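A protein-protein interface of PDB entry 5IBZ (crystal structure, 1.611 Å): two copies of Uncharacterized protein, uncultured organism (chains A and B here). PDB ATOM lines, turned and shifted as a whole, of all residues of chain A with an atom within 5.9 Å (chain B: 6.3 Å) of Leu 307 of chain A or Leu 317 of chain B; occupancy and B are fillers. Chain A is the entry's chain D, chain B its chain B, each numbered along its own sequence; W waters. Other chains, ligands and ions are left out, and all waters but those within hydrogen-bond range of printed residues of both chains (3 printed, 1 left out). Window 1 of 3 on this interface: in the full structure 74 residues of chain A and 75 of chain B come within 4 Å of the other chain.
O of Tyr 308 of chain A sits at hydrogen-bond distance from N of Ile 59 of chain B.
O of Ala 303 of chain B is in hydrogen-bond range of NE2 of Gln 305 of chain A (3.1 Å).
The side-chain amide oxygen (OE1) of Gln 305 of chain B is in hydrogen-bond range of the side-chain amide nitrogen (NE2) of Gln 305 of chain A (3.1 Å).
The backbone carbonyl oxygen of Lys 152 of chain A is in hydrogen-bond range of the side-chain amide nitrogen of Asn 318 of chain B.
O of Asn 318 of chain B lies within hydrogen-bond range of NE2 of Gln 305 of chain A (3.0 Å).
The backbone carbonyl oxygen of Pro 306 of chain A sits at hydrogen-bond distance from the side-chain amide nitrogen of Asn 318 of chain B, 2.8 Å away.
The backbone NH of Ile 57 of chain B lies within hydrogen-bond range of the side-chain hydroxyl of Thr 112 of chain B.
N of Leu 317 of chain B is in hydrogen-bond range of O of Thr 112 of chain B.
N of Leu 307 of chain B is in hydrogen-bond range of OG of Ser 315 of chain B (2.9 Å).
OG of Ser 315 of chain A is in hydrogen-bond range of N of Leu 307 of chain A.
Leu 317 of chain B touches Leu 307 of chain A.
Leu 307 of chain A touches Asn 318 of chain B (CD2 to N, 3.9 Å).
CD2 of Tyr 308 of chain A touches O of Ala 56 of chain B (3.4 Å).
Ile 57 of chain B touches Tyr 308 of chain A.
Ile 309 of chain A touches Ile 59 of chain B.
Leu 307 of chain B touches Leu 317 of chain A.
Printed residues of chain B within 4 Å of Gln 305 of chain A: Ala 303 (3.1 Å), Gln 305 (3.1 Å) and Asn 318 (3.0 Å).
Printed residues of chain A within 4 Å of Leu 307 of chain B: Leu 317.
Leu 317 of chain B touches just one residue of chain A: Leu 307.
The nearest residue of chain B that does not touch Leu 307 of chain A is Ile 59 of chain B (4.1 Å).
Of the 11 printed residues of chain A, 7 touch a printed residue of chain B.
Hydrophobic or aromatic side chains of chain A within 4 Å of the printed part of chain B: Leu 307, Tyr 308 and Ile 309.
Among the printed residues, no Asp or Glu carboxylate lies within 4 Å of a Lys or Arg side-chain nitrogen of the other chain.
Gln 305 of chain A touches its own counterpart, Gln 305 of chain B.
Leu 307 of chain A touches Leu 317 of chain B, and with the chains exchanged Leu 317 of chain A touches Leu 307 of chain B.
Positions printed for both chains: 305, 306, 307, 315, 316 and 317.
Of the 12 pairs that touch across the chains among the printed residues, 3 have their exchanged pair printed and touching as well.
Water W2 bridges the backbone carbonyl oxygen of Ala 56 of chain B and the side-chain amino group of Lys 152 of chain A.
Water W3 lies within hydrogen-bond range of O of Gln 305 of chain A (2.8 Å) and NE2 of Gln 305 of chain B (3.1 Å).
Water W1 lies within hydrogen-bond range of the backbone carbonyl oxygen (O) of Leu 317 of chain B (2.9 Å) and the backbone NH (N) of Tyr 308 of chain A (3.0 Å).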
ATOM      1  N   ILE A 148      -4.439 -18.548   6.606  1.00  0.00           N
ATOM      2  CA  ILE A 148      -5.601 -17.899   7.196  1.00  0.00           C
ATOM      3  C   ILE A 148      -6.362 -18.855   8.113  1.00  0.00           C
ATOM      4  O   ILE A 148      -7.148 -18.403   8.946  1.00  0.00           O
ATOM      5  CB  ILE A 148      -6.525 -17.315   6.093  1.00  0.00           C
ATOM      6  CG1 ILE A 148      -7.545 -16.303   6.651  1.00  0.00           C
ATOM      7  CG2 ILE A 148      -7.249 -18.440   5.320  1.00  0.00           C
ATOM      8  CD1 ILE A 148      -6.954 -14.917   6.969  1.00  0.00           C
ATOM      9  N   GLU A 149      -6.097 -20.157   8.031  1.00  0.00           N
ATOM     10  CA  GLU A 149      -6.781 -21.083   8.940  1.00  0.00           C
ATOM     11  C   GLU A 149      -6.408 -20.875  10.407  1.00  0.00           C
ATOM     12  O   GLU A 149      -7.134 -21.296  11.309  1.00  0.00           O
ATOM     13  CB  GLU A 149      -6.515 -22.552   8.544  1.00  0.00           C
ATOM     14  CG  GLU A 149      -5.160 -23.129   8.918  1.00  0.00           C
ATOM     15  CD  GLU A 149      -4.041 -22.784   7.969  1.00  0.00           C
ATOM     16  OE1 GLU A 149      -4.223 -21.952   7.050  1.00  0.00           O
ATOM     17  OE2 GLU A 149      -2.947 -23.361   8.165  1.00  0.00           O
ATOM     18  N   LYS A 152      -9.294 -18.894  11.910  1.00  0.00           N
ATOM     19  CA  LYS A 152     -10.642 -19.321  11.527  1.00  0.00           C
ATOM     20  C   LYS A 152     -11.722 -18.974  12.567  1.00  0.00           C
ATOM     21  O   LYS A 152     -12.902 -18.945  12.223  1.00  0.00           O
ATOM     22  CB  LYS A 152     -10.679 -20.824  11.243  1.00  0.00           C
ATOM     23  CG  LYS A 152     -10.532 -21.718  12.429  1.00  0.00           C
ATOM     24  CD  LYS A 152     -10.787 -23.173  12.055  1.00  0.00           C
ATOM     25  CE  LYS A 152     -10.688 -24.037  13.308  1.00  0.00           C
ATOM     26  NZ  LYS A 152     -11.151 -25.452  13.143  1.00  0.00           N
ATOM     27  N   GLN A 305     -15.470 -13.152  10.400  1.00  0.00           N
ATOM     28  CA  GLN A 305     -14.658 -14.348  10.295  1.00  0.00           C
ATOM     29  C   GLN A 305     -14.282 -14.650   8.841  1.00  0.00           C
ATOM     30  O   GLN A 305     -15.069 -14.431   7.928  1.00  0.00           O
ATOM     31  CB  GLN A 305     -15.399 -15.536  10.934  1.00  0.00           C
ATOM     32  CG  GLN A 305     -16.622 -16.060  10.206  1.00  0.00           C
ATOM     33  CD  GLN A 305     -17.920 -15.368  10.556  1.00  0.00           C
ATOM     34  OE1 GLN A 305     -17.952 -14.178  10.934  1.00  0.00           O
ATOM     35  NE2 GLN A 305     -19.016 -16.106  10.427  1.00  0.00           N
ATOM     36  N   PRO A 306     -13.067 -15.151   8.624  1.00  0.00           N
ATOM     37  CA  PRO A 306     -12.699 -15.617   7.294  1.00  0.00           C
ATOM     38  C   PRO A 306     -13.273 -16.986   7.006  1.00  0.00           C
ATOM     39  O   PRO A 306     -13.698 -17.666   7.952  1.00  0.00           O
ATOM     40  CB  PRO A 306     -11.177 -15.676   7.382  1.00  0.00           C
ATOM     41  CG  PRO A 306     -10.934 -16.141   8.754  1.00  0.00           C
ATOM     42  CD  PRO A 306     -12.017 -15.471   9.613  1.00  0.00           C
ATOM     43  N   LEU A 307     -13.265 -17.403   5.746  1.00  0.00           N
ATOM     44  CA  LEU A 307     -13.527 -18.793   5.435  1.00  0.00           C
ATOM     45  C   LEU A 307     -12.366 -19.647   5.942  1.00  0.00           C
ATOM     46  O   LEU A 307     -11.235 -19.182   6.053  1.00  0.00           O
ATOM     47  CB  LEU A 307     -13.719 -19.003   3.936  1.00  0.00           C
ATOM     48  CG  LEU A 307     -14.911 -18.291   3.300  1.00  0.00           C
ATOM     49  CD1 LEU A 307     -14.860 -18.508   1.804  1.00  0.00           C
ATOM     50  CD2 LEU A 307     -16.259 -18.747   3.901  1.00  0.00           C
ATOM     51  N   TYR A 308     -12.643 -20.915   6.233  1.00  0.00           N
ATOM     52  CA  TYR A 308     -11.626 -21.838   6.687  1.00  0.00           C
ATOM     53  C   TYR A 308     -10.916 -22.456   5.487  1.00  0.00           C
ATOM     54  O   TYR A 308     -11.350 -23.483   4.948  1.00  0.00           O
ATOM     55  CB  TYR A 308     -12.289 -22.894   7.563  1.00  0.00           C
ATOM     56  CG  TYR A 308     -11.411 -23.960   8.161  1.00  0.00           C
ATOM     57  CD1 TYR A 308     -10.045 -23.953   8.005  1.00  0.00           C
ATOM     58  CD2 TYR A 308     -11.985 -25.030   8.850  1.00  0.00           C
ATOM     59  CE1 TYR A 308      -9.264 -24.965   8.538  1.00  0.00           C
ATOM     60  CE2 TYR A 308     -11.211 -26.033   9.375  1.00  0.00           C
ATOM     61  CZ  TYR A 308      -9.865 -26.008   9.215  1.00  0.00           C
ATOM     62  OH  TYR A 308      -9.107 -27.035   9.752  1.00  0.00           O
ATOM     63  N   ILE A 309      -9.835 -21.812   5.038  1.00  0.00           N
ATOM     64  CA  ILE A 309      -9.130 -22.255   3.843  1.00  0.00           C
ATOM     65  C   ILE A 309      -7.681 -22.517   4.204  1.00  0.00           C
ATOM     66  O   ILE A 309      -6.869 -21.591   4.233  1.00  0.00           O
ATOM     67  CB  ILE A 309      -9.166 -21.212   2.698  1.00  0.00           C
ATOM     68  CG1 ILE A 309     -10.578 -20.634   2.506  1.00  0.00           C
ATOM     69  CG2 ILE A 309      -8.636 -21.837   1.424  1.00  0.00           C
ATOM     70  CD1 ILE A 309     -10.637 -19.493   1.491  1.00  0.00           C
ATOM     71  N   SER A 315      -8.876 -14.349   2.526  1.00  0.00           N
ATOM     72  CA  SER A 315     -10.199 -14.944   2.374  1.00  0.00           C
ATOM     73  C   SER A 315     -11.225 -13.904   1.982  1.00  0.00           C
ATOM     74  O   SER A 315     -11.191 -12.791   2.487  1.00  0.00           O
ATOM     75  CB  SER A 315     -10.633 -15.609   3.674  1.00  0.00           C
ATOM     76  OG  SER A 315     -11.906 -16.202   3.513  1.00  0.00           O
ATOM     77  N   PRO A 316     -12.166 -14.277   1.101  1.00  0.00           N
ATOM     78  CA  PRO A 316     -13.391 -13.488   1.009  1.00  0.00           C
ATOM     79  C   PRO A 316     -14.215 -13.601   2.279  1.00  0.00           C
ATOM     80  O   PRO A 316     -14.048 -14.519   3.085  1.00  0.00           O
ATOM     81  CB  PRO A 316     -14.139 -14.121  -0.178  1.00  0.00           C
ATOM     82  CG  PRO A 316     -13.651 -15.461  -0.257  1.00  0.00           C
ATOM     83  CD  PRO A 316     -12.222 -15.463   0.223  1.00  0.00           C
ATOM     84  N   LEU A 317     -15.134 -12.671   2.468  1.00  0.00           N
ATOM     85  CA  LEU A 317     -16.027 -12.778   3.601  1.00  0.00           C
ATOM     86  C   LEU A 317     -17.213 -11.885   3.404  1.00  0.00           C
ATOM     87  O   LEU A 317     -17.230 -11.073   2.485  1.00  0.00           O
ATOM     88  CB  LEU A 317     -15.322 -12.413   4.901  1.00  0.00           C
ATOM     89  CG  LEU A 317     -14.979 -10.949   5.133  1.00  0.00           C
ATOM     90  CD1 LEU A 317     -14.844 -10.723   6.650  1.00  0.00           C
ATOM     91  CD2 LEU A 317     -13.686 -10.587   4.431  1.00  0.00           C
ATOM     92  N   LEU B  55     -17.586 -24.030  12.826  1.00  0.00           N
ATOM     93  CA  LEU B  55     -18.321 -25.229  12.454  1.00  0.00           C
ATOM     94  C   LEU B  55     -18.103 -25.567  10.984  1.00  0.00           C
ATOM     95  O   LEU B  55     -18.942 -26.212  10.357  1.00  0.00           O
ATOM     96  CB  LEU B  55     -19.826 -25.052  12.749  1.00  0.00           C
ATOM     97  CG  LEU B  55     -20.129 -24.457  14.132  1.00  0.00           C
ATOM     98  CD1 LEU B  55     -21.641 -24.378  14.326  1.00  0.00           C
ATOM     99  CD2 LEU B  55     -19.523 -25.277  15.248  1.00  0.00           C
ATOM    100  N   ALA B  56     -16.975 -25.137  10.443  1.00  0.00           N
ATOM    101  CA  ALA B  56     -16.621 -25.446   9.061  1.00  0.00           C
ATOM    102  C   ALA B  56     -15.610 -26.575   8.937  1.00  0.00           C
ATOM    103  O   ALA B  56     -14.731 -26.741   9.786  1.00  0.00           O
ATOM    104  CB  ALA B  56     -16.072 -24.205   8.377  1.00  0.00           C
ATOM    105  N   ILE B  57     -15.717 -27.313   7.847  1.00  0.00           N
ATOM    106  CA  ILE B  57     -14.610 -28.168   7.407  1.00  0.00           C
ATOM    107  C   ILE B  57     -13.626 -27.314   6.607  1.00  0.00           C
ATOM    108  O   ILE B  57     -13.974 -26.247   6.090  1.00  0.00           O
ATOM    109  CB  ILE B  57     -15.076 -29.364   6.561  1.00  0.00           C
ATOM    110  CG1 ILE B  57     -15.800 -28.939   5.280  1.00  0.00           C
ATOM    111  CG2 ILE B  57     -15.942 -30.278   7.389  1.00  0.00           C
ATOM    112  CD1 ILE B  57     -15.789 -30.036   4.202  1.00  0.00           C
ATOM    113  N   ILE B  59     -11.736 -25.851   3.577  1.00  0.00           N
ATOM    114  CA  ILE B  59     -11.900 -25.731   2.130  1.00  0.00           C
ATOM    115  C   ILE B  59     -10.590 -26.141   1.476  1.00  0.00           C
ATOM    116  O   ILE B  59      -9.607 -25.390   1.493  1.00  0.00           O
ATOM    117  CB  ILE B  59     -12.280 -24.326   1.706  1.00  0.00           C
ATOM    118  CG1 ILE B  59     -13.619 -23.928   2.359  1.00  0.00           C
ATOM    119  CG2 ILE B  59     -12.358 -24.225   0.179  1.00  0.00           C
ATOM    120  CD1 ILE B  59     -14.127 -22.569   2.018  1.00  0.00           C
ATOM    121  N   MET B 106     -14.432 -23.443  -6.879  1.00  0.00           N
ATOM    122  CA  MET B 106     -15.192 -24.428  -6.126  1.00  0.00           C
ATOM    123  C   MET B 106     -16.662 -24.430  -6.445  1.00  0.00           C
ATOM    124  O   MET B 106     -17.221 -23.397  -6.848  1.00  0.00           O
ATOM    125  CB  MET B 106     -15.028 -24.181  -4.619  1.00  0.00           C
ATOM    126  CG  MET B 106     -15.609 -22.879  -4.161  1.00  0.00           C
ATOM    127  SD  MET B 106     -15.274 -22.531  -2.270  1.00  0.00           S
ATOM    128  CE  MET B 106     -16.323 -23.926  -1.426  1.00  0.00           C
ATOM    129  N   SER B 111     -18.635 -27.497  -0.021  1.00  0.00           N
ATOM    130  CA  SER B 111     -18.030 -27.498   1.307  1.00  0.00           C
ATOM    131  C   SER B 111     -19.116 -27.207   2.346  1.00  0.00           C
ATOM    132  O   SER B 111     -20.296 -27.330   2.053  1.00  0.00           O
ATOM    133  CB  SER B 111     -16.890 -26.475   1.383  1.00  0.00           C
ATOM    134  OG  SER B 111     -16.079 -26.669   2.530  1.00  0.00           O
ATOM    135  N   THR B 112     -18.734 -26.827   3.563  1.00  0.00           N
ATOM    136  CA  THR B 112     -19.694 -26.288   4.522  1.00  0.00           C
ATOM    137  C   THR B 112     -20.530 -25.225   3.811  1.00  0.00           C
ATOM    138  O   THR B 112     -19.984 -24.335   3.168  1.00  0.00           O
ATOM    139  CB  THR B 112     -18.971 -25.701   5.740  1.00  0.00           C
ATOM    140  OG1 THR B 112     -18.164 -26.731   6.342  1.00  0.00           O
ATOM    141  CG2 THR B 112     -19.954 -25.130   6.725  1.00  0.00           C
ATOM    142  N   GLN B 113     -21.850 -25.320   3.923  1.00  0.00           N
ATOM    143  CA  GLN B 113     -22.716 -24.539   3.048  1.00  0.00           C
ATOM    144  C   GLN B 113     -24.078 -24.230   3.627  1.00  0.00           C
ATOM    145  O   GLN B 113     -24.580 -24.955   4.499  1.00  0.00           O
ATOM    146  CB  GLN B 113     -22.920 -25.290   1.720  1.00  0.00           C
ATOM    147  CG  GLN B 113     -23.801 -26.541   1.846  1.00  0.00           C
ATOM    148  CD  GLN B 113     -23.709 -27.433   0.631  1.00  0.00           C
ATOM    149  OE1 GLN B 113     -24.604 -27.489  -0.207  1.00  0.00           O
ATOM    150  NE2 GLN B 113     -22.592 -28.092   0.508  1.00  0.00           N
ATOM    151  N   TRP B 114     -24.663 -23.160   3.098  1.00  0.00           N
ATOM    152  CA  TRP B 114     -26.121 -22.969   3.074  1.00  0.00           C
ATOM    153  C   TRP B 114     -26.590 -23.195   1.648  1.00  0.00           C
ATOM    154  O   TRP B 114     -25.924 -22.766   0.698  1.00  0.00           O
ATOM    155  CB  TRP B 114     -26.564 -21.568   3.474  1.00  0.00           C
ATOM    156  CG  TRP B 114     -26.571 -21.255   4.908  1.00  0.00           C
ATOM    157  CD1 TRP B 114     -25.848 -20.283   5.512  1.00  0.00           C
ATOM    158  CD2 TRP B 114     -27.362 -21.864   5.937  1.00  0.00           C
ATOM    159  NE1 TRP B 114     -26.131 -20.240   6.853  1.00  0.00           N
ATOM    160  CE2 TRP B 114     -27.055 -21.200   7.145  1.00  0.00           C
ATOM    161  CE3 TRP B 114     -28.283 -22.899   5.962  1.00  0.00           C
ATOM    162  CZ2 TRP B 114     -27.623 -21.552   8.351  1.00  0.00           C
ATOM    163  CZ3 TRP B 114     -28.870 -23.234   7.160  1.00  0.00           C
ATOM    164  CH2 TRP B 114     -28.528 -22.569   8.346  1.00  0.00           C
ATOM    165  N   GLU B 281     -25.351 -27.895   5.092  1.00  0.00           N
ATOM    166  CA  GLU B 281     -24.744 -29.210   4.930  1.00  0.00           C
ATOM    167  C   GLU B 281     -23.246 -29.157   5.115  1.00  0.00           C
ATOM    168  O   GLU B 281     -22.613 -28.124   4.864  1.00  0.00           O
ATOM    169  CB  GLU B 281     -25.063 -29.794   3.546  1.00  0.00           C
ATOM    170  CG  GLU B 281     -26.550 -30.093   3.384  1.00  0.00           C
ATOM    171  CD  GLU B 281     -26.986 -30.354   1.957  1.00  0.00           C
ATOM    172  OE1 GLU B 281     -26.267 -29.991   1.009  1.00  0.00           O
ATOM    173  OE2 GLU B 281     -28.067 -30.958   1.813  1.00  0.00           O
ATOM    174  N   TRP B 283     -21.458 -29.275   7.805  1.00  0.00           N
ATOM    175  CA  TRP B 283     -20.937 -28.555   8.960  1.00  0.00           C
ATOM    176  C   TRP B 283     -20.107 -29.512   9.822  1.00  0.00           C
ATOM    177  O   TRP B 283     -20.236 -30.737   9.707  1.00  0.00           O
ATOM    178  CB  TRP B 283     -22.089 -27.928   9.774  1.00  0.00           C
ATOM    179  CG  TRP B 283     -22.836 -26.810   9.074  1.00  0.00           C
ATOM    180  CD1 TRP B 283     -23.085 -26.693   7.739  1.00  0.00           C
ATOM    181  CD2 TRP B 283     -23.435 -25.664   9.693  1.00  0.00           C
ATOM    182  NE1 TRP B 283     -23.807 -25.544   7.482  1.00  0.00           N
ATOM    183  CE2 TRP B 283     -24.030 -24.894   8.667  1.00  0.00           C
ATOM    184  CE3 TRP B 283     -23.513 -25.205  11.012  1.00  0.00           C
ATOM    185  CZ2 TRP B 283     -24.711 -23.713   8.927  1.00  0.00           C
ATOM    186  CZ3 TRP B 283     -24.192 -24.027  11.267  1.00  0.00           C
ATOM    187  CH2 TRP B 283     -24.775 -23.297  10.236  1.00  0.00           C
ATOM    188  N   ALA B 303     -23.116 -17.048  14.177  1.00  0.00           N
ATOM    189  CA  ALA B 303     -22.829 -16.191  13.032  1.00  0.00           C
ATOM    190  C   ALA B 303     -22.581 -17.070  11.833  1.00  0.00           C
ATOM    191  O   ALA B 303     -21.457 -17.580  11.651  1.00  0.00           O
ATOM    192  CB  ALA B 303     -21.624 -15.301  13.300  1.00  0.00           C
ATOM    193  N   ALA B 304     -23.635 -17.268  11.036  1.00  0.00           N
ATOM    194  CA  ALA B 304     -23.596 -18.172   9.894  1.00  0.00           C
ATOM    195  C   ALA B 304     -24.060 -17.455   8.631  1.00  0.00           C
ATOM    196  O   ALA B 304     -24.740 -18.026   7.768  1.00  0.00           O
ATOM    197  CB  ALA B 304     -24.424 -19.395  10.166  1.00  0.00           C
ATOM    198  N   GLN B 305     -23.586 -16.234   8.462  1.00  0.00           N
ATOM    199  CA  GLN B 305     -23.948 -15.458   7.275  1.00  0.00           C
ATOM    200  C   GLN B 305     -23.359 -16.084   6.005  1.00  0.00           C
ATOM    201  O   GLN B 305     -22.250 -16.613   6.006  1.00  0.00           O
ATOM    202  CB  GLN B 305     -23.491 -14.002   7.438  1.00  0.00           C
ATOM    203  CG  GLN B 305     -21.965 -13.780   7.431  1.00  0.00           C
ATOM    204  CD  GLN B 305     -21.291 -13.865   8.813  1.00  0.00           C
ATOM    205  OE1 GLN B 305     -21.681 -14.656   9.677  1.00  0.00           O
ATOM    206  NE2 GLN B 305     -20.241 -13.077   8.991  1.00  0.00           N
ATOM    207  N   PRO B 306     -24.119 -16.034   4.913  1.00  0.00           N
ATOM    208  CA  PRO B 306     -23.562 -16.474   3.640  1.00  0.00           C
ATOM    209  C   PRO B 306     -22.683 -15.394   3.027  1.00  0.00           C
ATOM    210  O   PRO B 306     -22.720 -14.243   3.467  1.00  0.00           O
ATOM    211  CB  PRO B 306     -24.805 -16.678   2.781  1.00  0.00           C
ATOM    212  CG  PRO B 306     -25.700 -15.571   3.232  1.00  0.00           C
ATOM    213  CD  PRO B 306     -25.450 -15.420   4.735  1.00  0.00           C
ATOM    214  N   LEU B 307     -21.897 -15.753   2.024  1.00  0.00           N
ATOM    215  CA  LEU B 307     -21.231 -14.733   1.207  1.00  0.00           C
ATOM    216  C   LEU B 307     -22.283 -13.973   0.393  1.00  0.00           C
ATOM    217  O   LEU B 307     -23.344 -14.513   0.056  1.00  0.00           O
ATOM    218  CB  LEU B 307     -20.208 -15.341   0.261  1.00  0.00           C
ATOM    219  CG  LEU B 307     -19.048 -16.081   0.920  1.00  0.00           C
ATOM    220  CD1 LEU B 307     -18.172 -16.692  -0.135  1.00  0.00           C
ATOM    221  CD2 LEU B 307     -18.228 -15.121   1.801  1.00  0.00           C
ATOM    222  N   SER B 315     -24.108 -20.858  -0.715  1.00  0.00           N
ATOM    223  CA  SER B 315     -22.848 -20.223  -0.383  1.00  0.00           C
ATOM    224  C   SER B 315     -22.023 -21.076   0.550  1.00  0.00           C
ATOM    225  O   SER B 315     -22.587 -21.725   1.428  1.00  0.00           O
ATOM    226  CB  SER B 315     -23.104 -18.897   0.307  1.00  0.00           C
ATOM    227  OG  SER B 315     -21.889 -18.279   0.670  1.00  0.00           O
ATOM    228  N   PRO B 316     -20.692 -21.036   0.403  1.00  0.00           N
ATOM    229  CA  PRO B 316     -19.822 -21.504   1.479  1.00  0.00           C
ATOM    230  C   PRO B 316     -19.892 -20.550   2.643  1.00  0.00           C
ATOM    231  O   PRO B 316     -20.344 -19.406   2.520  1.00  0.00           O
ATOM    232  CB  PRO B 316     -18.420 -21.525   0.844  1.00  0.00           C
ATOM    233  CG  PRO B 316     -18.498 -20.638  -0.285  1.00  0.00           C
ATOM    234  CD  PRO B 316     -19.921 -20.586  -0.767  1.00  0.00           C
ATOM    235  N   LEU B 317     -19.487 -21.037   3.800  1.00  0.00           N
ATOM    236  CA  LEU B 317     -19.403 -20.161   4.954  1.00  0.00           C
ATOM    237  C   LEU B 317     -18.519 -20.768   6.016  1.00  0.00           C
ATOM    238  O   LEU B 317     -18.064 -21.896   5.899  1.00  0.00           O
ATOM    239  CB  LEU B 317     -20.780 -19.874   5.515  1.00  0.00           C
ATOM    240  CG  LEU B 317     -21.436 -21.043   6.224  1.00  0.00           C
ATOM    241  CD1 LEU B 317     -22.398 -20.484   7.299  1.00  0.00           C
ATOM    242  CD2 LEU B 317     -22.206 -21.892   5.264  1.00  0.00           C
ATOM    243  N   ASN B 318     -18.266 -19.952   7.039  1.00  0.00           N
ATOM    244  CA  ASN B 318     -17.583 -20.396   8.238  1.00  0.00           C
ATOM    245  C   ASN B 318     -18.484 -20.045   9.414  1.00  0.00           C
ATOM    246  O   ASN B 318     -18.383 -18.967   9.992  1.00  0.00           O
ATOM    247  CB  ASN B 318     -16.221 -19.741   8.365  1.00  0.00           C
ATOM    248  CG  ASN B 318     -15.485 -20.199   9.575  1.00  0.00           C
ATOM    249  OD1 ASN B 318     -15.896 -21.138  10.239  1.00  0.00           O
ATOM    250  ND2 ASN B 318     -14.402 -19.525   9.893  1.00  0.00           N
ATOM    251  N   PRO B 319     -19.415 -20.941   9.746  1.00  0.00           N
ATOM    252  CA  PRO B 319     -20.311 -20.603  10.870  1.00  0.00           C
ATOM    253  C   PRO B 319     -19.557 -20.569  12.196  1.00  0.00           C
ATOM    254  O   PRO B 319     -18.808 -21.523  12.469  1.00  0.00           O
ATOM    255  CB  PRO B 319     -21.338 -21.748  10.862  1.00  0.00           C
ATOM    256  CG  PRO B 319     -20.987 -22.615   9.672  1.00  0.00           C
ATOM    257  CD  PRO B 319     -19.560 -22.334   9.334  1.00  0.00           C
HETATM  258  O   HOH W   1     -15.233 -22.163   5.519  1.00  0.00           O
HETATM  259  O   HOH W   2     -13.793 -26.225  12.314  1.00  0.00           O
HETATM  260  O   HOH W   3     -17.417 -12.997   7.621  1.00  0.00           O
